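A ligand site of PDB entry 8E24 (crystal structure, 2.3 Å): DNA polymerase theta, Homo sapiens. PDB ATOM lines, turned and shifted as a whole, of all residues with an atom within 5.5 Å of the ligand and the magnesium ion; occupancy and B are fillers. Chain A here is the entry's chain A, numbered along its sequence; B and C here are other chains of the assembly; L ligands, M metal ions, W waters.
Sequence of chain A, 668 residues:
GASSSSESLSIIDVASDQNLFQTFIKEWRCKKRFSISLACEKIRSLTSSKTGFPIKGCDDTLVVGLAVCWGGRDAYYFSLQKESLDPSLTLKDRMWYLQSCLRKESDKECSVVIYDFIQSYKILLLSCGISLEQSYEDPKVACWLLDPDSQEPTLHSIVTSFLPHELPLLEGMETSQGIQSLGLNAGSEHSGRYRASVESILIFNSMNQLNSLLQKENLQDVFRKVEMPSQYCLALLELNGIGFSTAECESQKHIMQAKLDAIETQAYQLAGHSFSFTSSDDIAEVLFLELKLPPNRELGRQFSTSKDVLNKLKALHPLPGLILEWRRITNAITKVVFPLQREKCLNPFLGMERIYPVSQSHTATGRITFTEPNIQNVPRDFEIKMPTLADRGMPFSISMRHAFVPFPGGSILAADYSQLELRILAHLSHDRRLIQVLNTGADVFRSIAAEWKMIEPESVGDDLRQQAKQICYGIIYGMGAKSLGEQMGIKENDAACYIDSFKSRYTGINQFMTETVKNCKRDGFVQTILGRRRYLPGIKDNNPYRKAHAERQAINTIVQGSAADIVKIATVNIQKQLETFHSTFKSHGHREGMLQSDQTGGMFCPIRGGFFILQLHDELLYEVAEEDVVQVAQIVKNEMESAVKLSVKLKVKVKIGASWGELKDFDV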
ATOM      1  N   ARG A 367     -12.729  -5.498 -32.020  1.00  0.00           N
ATOM      2  CA  ARG A 367     -13.780  -6.209 -32.711  1.00  0.00           C
ATOM      3  C   ARG A 367     -14.444  -5.309 -33.748  1.00  0.00           C
ATOM      4  O   ARG A 367     -14.314  -4.082 -33.716  1.00  0.00           O
ATOM      5  CB  ARG A 367     -14.836  -6.714 -31.730  1.00  0.00           C
ATOM      6  CG  ARG A 367     -14.433  -7.962 -30.958  1.00  0.00           C
ATOM      7  CD  ARG A 367     -15.598  -8.467 -30.120  1.00  0.00           C
ATOM      8  NE  ARG A 367     -15.385  -9.830 -29.653  1.00  0.00           N
ATOM      9  CZ  ARG A 367     -16.328 -10.595 -29.121  1.00  0.00           C
ATOM     10  NH1 ARG A 367     -17.571 -10.151 -28.986  1.00  0.00           N
ATOM     11  NH2 ARG A 367     -16.030 -11.822 -28.729  1.00  0.00           N
ATOM     12  N   ARG A 380     -30.589 -16.070 -32.153  1.00  0.00           N
ATOM     13  CA  ARG A 380     -30.345 -17.480 -32.406  1.00  0.00           C
ATOM     14  C   ARG A 380     -31.664 -18.202 -32.679  1.00  0.00           C
ATOM     15  O   ARG A 380     -32.748 -17.707 -32.381  1.00  0.00           O
ATOM     16  CB  ARG A 380     -29.644 -18.135 -31.221  1.00  0.00           C
ATOM     17  CG  ARG A 380     -28.321 -17.508 -30.822  1.00  0.00           C
ATOM     18  CD  ARG A 380     -27.759 -18.179 -29.566  1.00  0.00           C
ATOM     19  NE  ARG A 380     -27.413 -19.576 -29.787  1.00  0.00           N
ATOM     20  CZ  ARG A 380     -26.200 -20.017 -30.083  1.00  0.00           C
ATOM     21  NH1 ARG A 380     -25.179 -19.183 -30.209  1.00  0.00           N
ATOM     22  NH2 ARG A 380     -26.000 -21.312 -30.260  1.00  0.00           N
ATOM     23  N   ASP A 416     -15.851 -20.438 -39.180  1.00  0.00           N
ATOM     24  CA  ASP A 416     -15.644 -19.943 -37.832  1.00  0.00           C
ATOM     25  C   ASP A 416     -14.472 -20.654 -37.179  1.00  0.00           C
ATOM     26  O   ASP A 416     -14.236 -21.840 -37.414  1.00  0.00           O
ATOM     27  CB  ASP A 416     -16.898 -20.114 -36.965  1.00  0.00           C
ATOM     28  CG  ASP A 416     -17.252 -21.574 -36.742  1.00  0.00           C
ATOM     29  OD1 ASP A 416     -17.190 -22.358 -37.710  1.00  0.00           O
ATOM     30  OD2 ASP A 416     -17.580 -21.937 -35.588  1.00  0.00           O
ATOM     31  N   TYR A 417     -13.743 -19.907 -36.342  1.00  0.00           N
ATOM     32  CA  TYR A 417     -12.680 -20.507 -35.545  1.00  0.00           C
ATOM     33  C   TYR A 417     -13.289 -21.333 -34.413  1.00  0.00           C
ATOM     34  O   TYR A 417     -14.295 -20.944 -33.810  1.00  0.00           O
ATOM     35  CB  TYR A 417     -11.772 -19.418 -34.971  1.00  0.00           C
ATOM     36  CG  TYR A 417     -10.800 -18.811 -35.952  1.00  0.00           C
ATOM     37  CD1 TYR A 417      -9.680 -19.515 -36.366  1.00  0.00           C
ATOM     38  CD2 TYR A 417     -10.984 -17.529 -36.443  1.00  0.00           C
ATOM     39  CE1 TYR A 417      -8.775 -18.966 -37.260  1.00  0.00           C
ATOM     40  CE2 TYR A 417     -10.087 -16.970 -37.333  1.00  0.00           C
ATOM     41  CZ  TYR A 417      -8.987 -17.694 -37.736  1.00  0.00           C
ATOM     42  OH  TYR A 417      -8.087 -17.137 -38.616  1.00  0.00           O
ATOM     43  N   GLN A 419     -13.190 -22.199 -30.917  1.00  0.00           N
ATOM     44  CA  GLN A 419     -12.718 -21.708 -29.623  1.00  0.00           C
ATOM     45  C   GLN A 419     -11.437 -20.903 -29.774  1.00  0.00           C
ATOM     46  O   GLN A 419     -10.377 -21.240 -29.235  1.00  0.00           O
ATOM     47  CB  GLN A 419     -12.523 -22.876 -28.637  1.00  0.00           C
ATOM     48  CG  GLN A 419     -13.822 -23.439 -28.063  1.00  0.00           C
ATOM     49  CD  GLN A 419     -14.690 -24.098 -29.111  1.00  0.00           C
ATOM     50  OE1 GLN A 419     -14.269 -25.031 -29.798  1.00  0.00           O
ATOM     51  NE2 GLN A 419     -15.926 -23.618 -29.242  1.00  0.00           N
ATOM     52  N   GLU A 421     -10.647 -17.855 -28.671  1.00  0.00           N
ATOM     53  CA  GLU A 421     -10.142 -17.198 -27.464  1.00  0.00           C
ATOM     54  C   GLU A 421      -9.487 -18.183 -26.517  1.00  0.00           C
ATOM     55  O   GLU A 421      -8.497 -17.857 -25.862  1.00  0.00           O
ATOM     56  CB  GLU A 421     -11.268 -16.443 -26.765  1.00  0.00           C
ATOM     57  CG  GLU A 421     -11.824 -15.279 -27.582  1.00  0.00           C
ATOM     58  CD  GLU A 421     -12.649 -14.312 -26.741  1.00  0.00           C
ATOM     59  OE1 GLU A 421     -12.784 -14.548 -25.521  1.00  0.00           O
ATOM     60  OE2 GLU A 421     -13.166 -13.321 -27.310  1.00  0.00           O
ATOM     61  N   ASP A 443     -16.561 -31.189 -27.233  1.00  0.00           N
ATOM     62  CA  ASP A 443     -17.075 -29.850 -26.963  1.00  0.00           C
ATOM     63  C   ASP A 443     -16.860 -29.501 -25.492  1.00  0.00           C
ATOM     64  O   ASP A 443     -17.367 -30.201 -24.609  1.00  0.00           O
ATOM     65  CB  ASP A 443     -18.546 -29.747 -27.329  1.00  0.00           C
ATOM     66  CG  ASP A 443     -19.080 -28.330 -27.247  1.00  0.00           C
ATOM     67  OD1 ASP A 443     -18.700 -27.495 -28.103  1.00  0.00           O
ATOM     68  OD2 ASP A 443     -19.866 -28.039 -26.318  1.00  0.00           O
ATOM     69  N   PHE A 445     -18.098 -27.107 -23.808  1.00  0.00           N
ATOM     70  CA  PHE A 445     -19.319 -26.652 -23.140  1.00  0.00           C
ATOM     71  C   PHE A 445     -20.281 -27.801 -22.844  1.00  0.00           C
ATOM     72  O   PHE A 445     -20.994 -27.750 -21.836  1.00  0.00           O
ATOM     73  CB  PHE A 445     -19.988 -25.588 -24.004  1.00  0.00           C
ATOM     74  CG  PHE A 445     -19.076 -24.461 -24.367  1.00  0.00           C
ATOM     75  CD1 PHE A 445     -18.198 -23.933 -23.444  1.00  0.00           C
ATOM     76  CD2 PHE A 445     -19.069 -23.940 -25.653  1.00  0.00           C
ATOM     77  CE1 PHE A 445     -17.339 -22.896 -23.782  1.00  0.00           C
ATOM     78  CE2 PHE A 445     -18.213 -22.910 -26.003  1.00  0.00           C
ATOM     79  CZ  PHE A 445     -17.342 -22.396 -25.060  1.00  0.00           C
ATOM     80  N   ARG A 465     -26.191 -25.661 -23.261  1.00  0.00           N
ATOM     81  CA  ARG A 465     -24.838 -25.438 -23.753  1.00  0.00           C
ATOM     82  C   ARG A 465     -24.479 -23.953 -23.720  1.00  0.00           C
ATOM     83  O   ARG A 465     -23.353 -23.580 -23.361  1.00  0.00           O
ATOM     84  CB  ARG A 465     -24.684 -25.999 -25.168  1.00  0.00           C
ATOM     85  CG  ARG A 465     -23.275 -25.905 -25.721  1.00  0.00           C
ATOM     86  CD  ARG A 465     -23.182 -26.469 -27.133  1.00  0.00           C
ATOM     87  NE  ARG A 465     -21.818 -26.450 -27.639  1.00  0.00           N
ATOM     88  CZ  ARG A 465     -21.250 -25.400 -28.231  1.00  0.00           C
ATOM     89  NH1 ARG A 465     -21.913 -24.269 -28.401  1.00  0.00           N
ATOM     90  NH2 ARG A 465     -20.002 -25.503 -28.663  1.00  0.00           N
ATOM     91  N   GLN A 466     -25.425 -23.086 -24.100  1.00  0.00           N
ATOM     92  CA  GLN A 466     -25.206 -21.648 -23.992  1.00  0.00           C
ATOM     93  C   GLN A 466     -25.021 -21.230 -22.540  1.00  0.00           C
ATOM     94  O   GLN A 466     -24.190 -20.368 -22.238  1.00  0.00           O
ATOM     95  CB  GLN A 466     -26.370 -20.890 -24.626  1.00  0.00           C
ATOM     96  CG  GLN A 466     -26.372 -20.910 -26.141  1.00  0.00           C
ATOM     97  CD  GLN A 466     -25.187 -20.177 -26.726  1.00  0.00           C
ATOM     98  OE1 GLN A 466     -24.286 -20.793 -27.300  1.00  0.00           O
ATOM     99  NE2 GLN A 466     -25.174 -18.864 -26.575  1.00  0.00           N
ATOM    100  N   LYS A 469     -21.667 -22.082 -21.645  1.00  0.00           N
ATOM    101  CA  LYS A 469     -20.729 -21.199 -22.317  1.00  0.00           C
ATOM    102  C   LYS A 469     -20.518 -19.914 -21.537  1.00  0.00           C
ATOM    103  O   LYS A 469     -19.376 -19.442 -21.391  1.00  0.00           O
ATOM    104  CB  LYS A 469     -21.226 -20.887 -23.729  1.00  0.00           C
ATOM    105  CG  LYS A 469     -20.342 -19.901 -24.482  1.00  0.00           C
ATOM    106  CD  LYS A 469     -20.947 -19.497 -25.817  1.00  0.00           C
ATOM    107  CE  LYS A 469     -21.105 -20.690 -26.747  1.00  0.00           C
ATOM    108  NZ  LYS A 469     -21.599 -20.277 -28.096  1.00  0.00           N
ATOM    109  N   GLN A 470     -21.599 -19.328 -21.010  1.00  0.00           N
ATOM    110  CA  GLN A 470     -21.446 -18.136 -20.184  1.00  0.00           C
ATOM    111  C   GLN A 470     -20.783 -18.465 -18.847  1.00  0.00           C
ATOM    112  O   GLN A 470     -20.049 -17.646 -18.300  1.00  0.00           O
ATOM    113  CB  GLN A 470     -22.804 -17.480 -19.955  1.00  0.00           C
ATOM    114  CG  GLN A 470     -23.518 -17.072 -21.232  1.00  0.00           C
ATOM    115  CD  GLN A 470     -24.574 -16.013 -21.009  1.00  0.00           C
ATOM    116  OE1 GLN A 470     -24.676 -15.451 -19.921  1.00  0.00           O
ATOM    117  NE2 GLN A 470     -25.370 -15.744 -22.034  1.00  0.00           N
ATOM    118  N   TYR A 473     -16.749 -18.750 -20.026  1.00  0.00           N
ATOM    119  CA  TYR A 473     -16.058 -17.473 -20.211  1.00  0.00           C
ATOM    120  C   TYR A 473     -16.237 -16.563 -19.009  1.00  0.00           C
ATOM    121  O   TYR A 473     -15.349 -15.749 -18.709  1.00  0.00           O
ATOM    122  CB  TYR A 473     -16.559 -16.778 -21.476  1.00  0.00           C
ATOM    123  CG  TYR A 473     -16.261 -17.537 -22.747  1.00  0.00           C
ATOM    124  CD1 TYR A 473     -14.947 -17.720 -23.180  1.00  0.00           C
ATOM    125  CD2 TYR A 473     -17.278 -18.073 -23.524  1.00  0.00           C
ATOM    126  CE1 TYR A 473     -14.669 -18.413 -24.348  1.00  0.00           C
ATOM    127  CE2 TYR A 473     -17.009 -18.778 -24.682  1.00  0.00           C
ATOM    128  CZ  TYR A 473     -15.698 -18.944 -25.089  1.00  0.00           C
ATOM    129  OH  TYR A 473     -15.427 -19.639 -26.245  1.00  0.00           O
ATOM    130  N   GLY A 474     -17.361 -16.681 -18.297  1.00  0.00           N
ATOM    131  CA  GLY A 474     -17.550 -15.871 -17.104  1.00  0.00           C
ATOM    132  C   GLY A 474     -16.509 -16.157 -16.047  1.00  0.00           C
ATOM    133  O   GLY A 474     -15.835 -15.247 -15.560  1.00  0.00           O
ATOM    134  N   TYR A 477     -13.104 -14.983 -17.081  1.00  0.00           N
ATOM    135  CA  TYR A 477     -12.940 -13.533 -17.115  1.00  0.00           C
ATOM    136  C   TYR A 477     -13.395 -12.849 -15.823  1.00  0.00           C
ATOM    137  O   TYR A 477     -13.835 -11.701 -15.853  1.00  0.00           O
ATOM    138  CB  TYR A 477     -13.683 -12.951 -18.316  1.00  0.00           C
ATOM    139  CG  TYR A 477     -13.058 -13.353 -19.641  1.00  0.00           C
ATOM    140  CD1 TYR A 477     -11.717 -13.099 -19.903  1.00  0.00           C
ATOM    141  CD2 TYR A 477     -13.805 -13.979 -20.626  1.00  0.00           C
ATOM    142  CE1 TYR A 477     -11.130 -13.458 -21.104  1.00  0.00           C
ATOM    143  CE2 TYR A 477     -13.231 -14.344 -21.836  1.00  0.00           C
ATOM    144  CZ  TYR A 477     -11.900 -14.085 -22.063  1.00  0.00           C
ATOM    145  OH  TYR A 477     -11.323 -14.442 -23.262  1.00  0.00           O
ATOM    146  N   ASN A 556      -9.165  -9.644 -20.313  1.00  0.00           N
ATOM    147  CA  ASN A 556     -10.069  -9.930 -21.420  1.00  0.00           C
ATOM    148  C   ASN A 556      -9.633  -9.229 -22.706  1.00  0.00           C
ATOM    149  O   ASN A 556      -9.791  -9.776 -23.803  1.00  0.00           O
ATOM    150  CB  ASN A 556     -11.496  -9.536 -21.052  1.00  0.00           C
ATOM    151  CG  ASN A 556     -12.472  -9.736 -22.187  1.00  0.00           C
ATOM    152  OD1 ASN A 556     -12.730  -8.822 -22.970  1.00  0.00           O
ATOM    153  ND2 ASN A 556     -13.032 -10.936 -22.290  1.00  0.00           N
ATOM    154  N   GLN A 560      -9.446 -11.250 -26.129  1.00  0.00           N
ATOM    155  CA  GLN A 560     -10.470 -10.889 -27.102  1.00  0.00           C
ATOM    156  C   GLN A 560      -9.907  -9.993 -28.197  1.00  0.00           C
ATOM    157  O   GLN A 560     -10.268 -10.132 -29.370  1.00  0.00           O
ATOM    158  CB  GLN A 560     -11.643 -10.211 -26.397  1.00  0.00           C
ATOM    159  CG  GLN A 560     -12.806  -9.875 -27.300  1.00  0.00           C
ATOM    160  CD  GLN A 560     -13.873  -9.079 -26.585  1.00  0.00           C
ATOM    161  OE1 GLN A 560     -13.858  -7.849 -26.600  1.00  0.00           O
ATOM    162  NE2 GLN A 560     -14.802  -9.775 -25.938  1.00  0.00           N
ATOM    163  N   HIS A 617     -17.193 -11.835 -35.236  1.00  0.00           N
ATOM    164  CA  HIS A 617     -16.186 -11.891 -34.184  1.00  0.00           C
ATOM    165  C   HIS A 617     -15.266 -13.101 -34.323  1.00  0.00           C
ATOM    166  O   HIS A 617     -14.040 -12.945 -34.358  1.00  0.00           O
ATOM    167  CB  HIS A 617     -16.850 -11.872 -32.807  1.00  0.00           C
ATOM    168  CG  HIS A 617     -17.827 -10.746 -32.619  1.00  0.00           C
ATOM    169  ND1 HIS A 617     -19.131 -10.946 -32.229  1.00  0.00           N
ATOM    170  CD2 HIS A 617     -17.675  -9.414 -32.781  1.00  0.00           C
ATOM    171  CE1 HIS A 617     -19.750  -9.784 -32.150  1.00  0.00           C
ATOM    172  NE2 HIS A 617     -18.888  -8.840 -32.488  1.00  0.00           N
ATOM    173  N   ASP A 618     -15.834 -14.310 -34.373  1.00  0.00           N
ATOM    174  CA  ASP A 618     -15.060 -15.515 -34.603  1.00  0.00           C
ATOM    175  C   ASP A 618     -15.455 -16.224 -35.888  1.00  0.00           C
ATOM    176  O   ASP A 618     -14.999 -17.355 -36.132  1.00  0.00           O
ATOM    177  CB  ASP A 618     -15.191 -16.484 -33.414  1.00  0.00           C
ATOM    178  CG  ASP A 618     -16.509 -17.245 -33.423  1.00  0.00           C
ATOM    179  OD1 ASP A 618     -17.531 -16.691 -33.883  1.00  0.00           O
ATOM    180  OD2 ASP A 618     -16.517 -18.405 -32.955  1.00  0.00           O
ATOM    181  P    DC B   4     -19.446 -10.284 -11.459  1.00  0.00           P
ATOM    182  OP1  DC B   4     -20.843 -10.133 -11.916  1.00  0.00           O
ATOM    183  OP2  DC B   4     -19.152 -11.159 -10.298  1.00  0.00           O
ATOM    184  O5'  DC B   4     -18.557 -10.767 -12.694  1.00  0.00           O
ATOM    185  C5'  DC B   4     -18.575 -10.031 -13.908  1.00  0.00           C
ATOM    186  C4'  DC B   4     -17.463 -10.485 -14.844  1.00  0.00           C
ATOM    187  O4'  DC B   4     -17.756 -11.815 -15.320  1.00  0.00           O
ATOM    188  C3'  DC B   4     -17.307  -9.641 -16.096  1.00  0.00           C
ATOM    189  O3'  DC B   4     -16.455  -8.539 -15.831  1.00  0.00           O
ATOM    190  C2'  DC B   4     -16.652 -10.624 -17.069  1.00  0.00           C
ATOM    191  C1'  DC B   4     -17.265 -11.965 -16.643  1.00  0.00           C
ATOM    192  N1   DC B   4     -18.384 -12.429 -17.517  1.00  0.00           N
ATOM    193  C2   DC B   4     -18.106 -12.984 -18.771  1.00  0.00           C
ATOM    194  O2   DC B   4     -16.923 -13.081 -19.134  1.00  0.00           O
ATOM    195  N3   DC B   4     -19.134 -13.395 -19.550  1.00  0.00           N
ATOM    196  C4   DC B   4     -20.391 -13.282 -19.115  1.00  0.00           C
ATOM    197  N4   DC B   4     -21.374 -13.705 -19.918  1.00  0.00           N
ATOM    198  C5   DC B   4     -20.695 -12.717 -17.842  1.00  0.00           C
ATOM    199  C6   DC B   4     -19.672 -12.311 -17.084  1.00  0.00           C
ATOM    200  P    DC B   5     -16.757  -7.116 -16.506  1.00  0.00           P
ATOM    201  OP1  DC B   5     -15.877  -6.120 -15.850  1.00  0.00           O
ATOM    202  OP2  DC B   5     -18.227  -6.908 -16.493  1.00  0.00           O
ATOM    203  O5'  DC B   5     -16.298  -7.297 -18.027  1.00  0.00           O
ATOM    204  C5'  DC B   5     -14.917  -7.376 -18.348  1.00  0.00           C
ATOM    205  C4'  DC B   5     -14.725  -7.696 -19.815  1.00  0.00           C
ATOM    206  O4'  DC B   5     -15.278  -9.007 -20.101  1.00  0.00           O
ATOM    207  C3'  DC B   5     -15.441  -6.771 -20.782  1.00  0.00           C
ATOM    208  O3'  DC B   5     -14.636  -5.618 -21.041  1.00  0.00           O
ATOM    209  C2'  DC B   5     -15.578  -7.645 -22.017  1.00  0.00           C
ATOM    210  C1'  DC B   5     -15.782  -9.038 -21.426  1.00  0.00           C
ATOM    211  N1   DC B   5     -17.197  -9.476 -21.396  1.00  0.00           N
ATOM    212  C2   DC B   5     -17.772 -10.032 -22.544  1.00  0.00           C
ATOM    213  O2   DC B   5     -17.067 -10.163 -23.556  1.00  0.00           O
ATOM    214  N3   DC B   5     -19.069 -10.424 -22.511  1.00  0.00           N
ATOM    215  C4   DC B   5     -19.778 -10.269 -21.398  1.00  0.00           C
ATOM    216  N4   DC B   5     -21.056 -10.666 -21.412  1.00  0.00           N
ATOM    217  C5   DC B   5     -19.225  -9.695 -20.220  1.00  0.00           C
ATOM    218  C6   DC B   5     -17.942  -9.310 -20.262  1.00  0.00           C
ATOM    219  P    DG C  13     -24.843 -15.671 -31.051  1.00  0.00           P
ATOM    220  OP1  DG C  13     -24.921 -16.683 -32.129  1.00  0.00           O
ATOM    221  OP2  DG C  13     -25.335 -16.009 -29.695  1.00  0.00           O
ATOM    222  O5'  DG C  13     -23.338 -15.151 -30.917  1.00  0.00           O
ATOM    223  C5'  DG C  13     -22.646 -14.673 -32.059  1.00  0.00           C
ATOM    224  C4'  DG C  13     -21.362 -13.966 -31.675  1.00  0.00           C
ATOM    225  O4'  DG C  13     -21.656 -12.862 -30.783  1.00  0.00           O
ATOM    226  C3'  DG C  13     -20.360 -14.808 -30.916  1.00  0.00           C
ATOM    227  C2'  DG C  13     -19.523 -13.745 -30.204  1.00  0.00           C
ATOM    228  C1'  DG C  13     -20.564 -12.665 -29.886  1.00  0.00           C
ATOM    229  N9   DG C  13     -21.071 -12.726 -28.521  1.00  0.00           N
ATOM    230  C8   DG C  13     -22.234 -13.309 -28.098  1.00  0.00           C
ATOM    231  N7   DG C  13     -22.428 -13.211 -26.814  1.00  0.00           N
ATOM    232  C5   DG C  13     -21.322 -12.516 -26.350  1.00  0.00           C
ATOM    233  C6   DG C  13     -20.977 -12.103 -25.042  1.00  0.00           C
ATOM    234  O6   DG C  13     -21.605 -12.286 -23.989  1.00  0.00           O
ATOM    235  N1   DG C  13     -19.765 -11.424 -25.015  1.00  0.00           N
ATOM    236  C2   DG C  13     -18.977 -11.171 -26.112  1.00  0.00           C
ATOM    237  N2   DG C  13     -17.839 -10.488 -25.888  1.00  0.00           N
ATOM    238  N3   DG C  13     -19.289 -11.541 -27.345  1.00  0.00           N
ATOM    239  C4   DG C  13     -20.475 -12.209 -27.397  1.00  0.00           C
HETATM  240  P1  LIG L   1     -19.546 -22.326 -30.559  1.00  0.00           P
HETATM  241  O1  LIG L   1     -18.348 -23.235 -30.636  1.00  0.00           O
HETATM  242  O2  LIG L   1     -20.827 -23.026 -30.196  1.00  0.00           O
HETATM  243  O3  LIG L   1     -19.672 -21.342 -31.704  1.00  0.00           O
HETATM  244  O4  LIG L   1     -19.240 -21.388 -29.287  1.00  0.00           O
HETATM  245  P2  LIG L   1     -17.891 -20.503 -29.196  1.00  0.00           P
HETATM  246  O5  LIG L   1     -17.027 -21.062 -28.092  1.00  0.00           O
HETATM  247  O6  LIG L   1     -17.307 -20.336 -30.579  1.00  0.00           O
HETATM  248  O7  LIG L   1     -18.489 -19.121 -28.656  1.00  0.00           O
HETATM  249  P3  LIG L   1     -19.146 -18.000 -29.616  1.00  0.00           P
HETATM  250  O8  LIG L   1     -20.584 -17.847 -29.213  1.00  0.00           O
HETATM  251  O9  LIG L   1     -18.801 -18.250 -31.072  1.00  0.00           O
HETATM  252  O10 LIG L   1     -18.333 -16.711 -29.113  1.00  0.00           O
HETATM  253  C1  LIG L   1     -17.166 -16.289 -29.833  1.00  0.00           C
HETATM  254  C2  LIG L   1     -16.269 -15.537 -28.866  1.00  0.00           C
HETATM  255  O11 LIG L   1     -17.049 -14.598 -28.126  1.00  0.00           O
HETATM  256  C3  LIG L   1     -15.670 -16.505 -27.860  1.00  0.00           C
HETATM  257  C4  LIG L   1     -15.749 -15.796 -26.526  1.00  0.00           C
HETATM  258  C5  LIG L   1     -16.680 -14.611 -26.746  1.00  0.00           C
HETATM  259  N1  LIG L   1     -17.878 -14.784 -25.903  1.00  0.00           N
HETATM  260  C6  LIG L   1     -19.034 -15.377 -26.271  1.00  0.00           C
HETATM  261  N2  LIG L   1     -19.925 -15.377 -25.253  1.00  0.00           N
HETATM  262  C7  LIG L   1     -19.340 -14.773 -24.203  1.00  0.00           C
HETATM  263  C8  LIG L   1     -19.725 -14.434 -22.812  1.00  0.00           C
HETATM  264  O12 LIG L   1     -20.858 -14.728 -22.366  1.00  0.00           O
HETATM  265  N3  LIG L   1     -18.818 -13.799 -22.051  1.00  0.00           N
HETATM  266  C9  LIG L   1     -17.591 -13.475 -22.502  1.00  0.00           C
HETATM  267  N4  LIG L   1     -16.738 -12.835 -21.674  1.00  0.00           N
HETATM  268  N5  LIG L   1     -17.177 -13.750 -23.760  1.00  0.00           N
HETATM  269  C10 LIG L   1     -17.990 -14.386 -24.638  1.00  0.00           C
HETATM  270 MG    MG M   1     -17.742 -20.019 -32.402  1.00  0.00          MG
HETATM  271  O   HOH W   1     -13.548 -14.026 -30.140  1.00  0.00           O
HETATM  272  O   HOH W   2     -21.610 -20.623 -34.442  1.00  0.00           O
HETATM  273  O   HOH W   3     -15.102 -19.152 -31.045  1.00  0.00           O
HETATM  274  O   HOH W   4     -16.296 -24.029 -32.002  1.00  0.00           O
HETATM  275  O   HOH W   5     -19.329 -18.790 -33.634  1.00  0.00           O
HETATM  276  O   HOH W   6     -23.482 -14.510 -23.727  1.00  0.00           O
HETATM  277  O   HOH W   7     -21.617 -18.615 -32.470  1.00  0.00           O
HETATM  278  O   HOH W   8     -13.342 -17.565 -29.925  1.00  0.00           O
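OD2 of Asp 416 touches the magnesium ion, at 3.7 Å.
Tyr 417 touches the magnesium ion (O to MG, 3.8 Å).
Of the 22 residues printed, 3 come within 4 Å of the magnesium ion.
O6 of DG 13 of chain C lies close to an oxygen (O12) of the ligand (3.0 Å).
Merely in contact with the ligand: Glu 421 (3.4 Å), Phe 445 (3.0 Å), Gln 470 (3.7 Å) and Tyr 477 (3.3 Å).
The nearest printed residue that does not touch the ligand is Asn 556 (4.2 Å).
N2 of DG 13 of chain C is in hydrogen-bond range of the side-chain amide nitrogen (NE2) of Gln 560.
The side-chain amide oxygen of Gln 466 lies within hydrogen-bond range of the side-chain amino group of Lys 469, 2.8 Å away.
A ring nitrogen (ND1) of His 617 sits close to O4' of DG 13 of chain C (3.5 Å).
N2 of DG 13 of chain C lies close to O2 of DC 5 of chain B, at 2.5 Å.
NE2 of Gln 560 sits at hydrogen-bond distance from O2 of DC 5 of chain B, 3.3 Å away.
OP1 of DG 13 of chain C lies within salt-bridge range of NH1 of Arg 380 (3.2 Å).
The side-chain carboxylate (OD2) of Asp 443 lies close to the backbone NH (N) of Phe 445.
NH2 of Arg 465 lies within salt-bridge range of OD1 of Asp 443 (2.4 Å).
O2 of DC 5 of chain B sits close to a nitrogen (N4) of the ligand, 3.3 Å away.
N3 of the ligand sits at hydrogen-bond distance from N3 of DC 4 of chain B (2.6 Å).
O11 of the ligand is in hydrogen-bond range of NH2 of Arg 367 (3.0 Å).
OH of Tyr 473 lies within hydrogen-bond range of O5 of the ligand.
NZ of Lys 469 lies within salt-bridge range of O8 of the ligand, at 2.9 Å.
The guanidinium group (NH1) of Arg 465 is in salt-bridge range of an oxygen (O2) of the ligand (2.4 Å).
The side-chain amide nitrogen (NE2) of Gln 419 lies within hydrogen-bond range of an oxygen (O1) of the ligand (2.8 Å).
Water W4 bridges an oxygen (O1) of the ligand and the side-chain amide nitrogen (NE2) of Gln 419.
Water W6 lies within hydrogen-bond range of the side-chain amide nitrogen (NE2) of Gln 470 (2.8 Å), O6 of DG 13 of chain C (2.9 Å) and an oxygen (O12) of the ligand (3.0 Å).
The magnesium ion is bound by O6 of the ligand, OD2 of Asp 618, water W5, O3 of the ligand and O9 of the ligand.
The magnesium ion has five donor atoms within binding distance.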
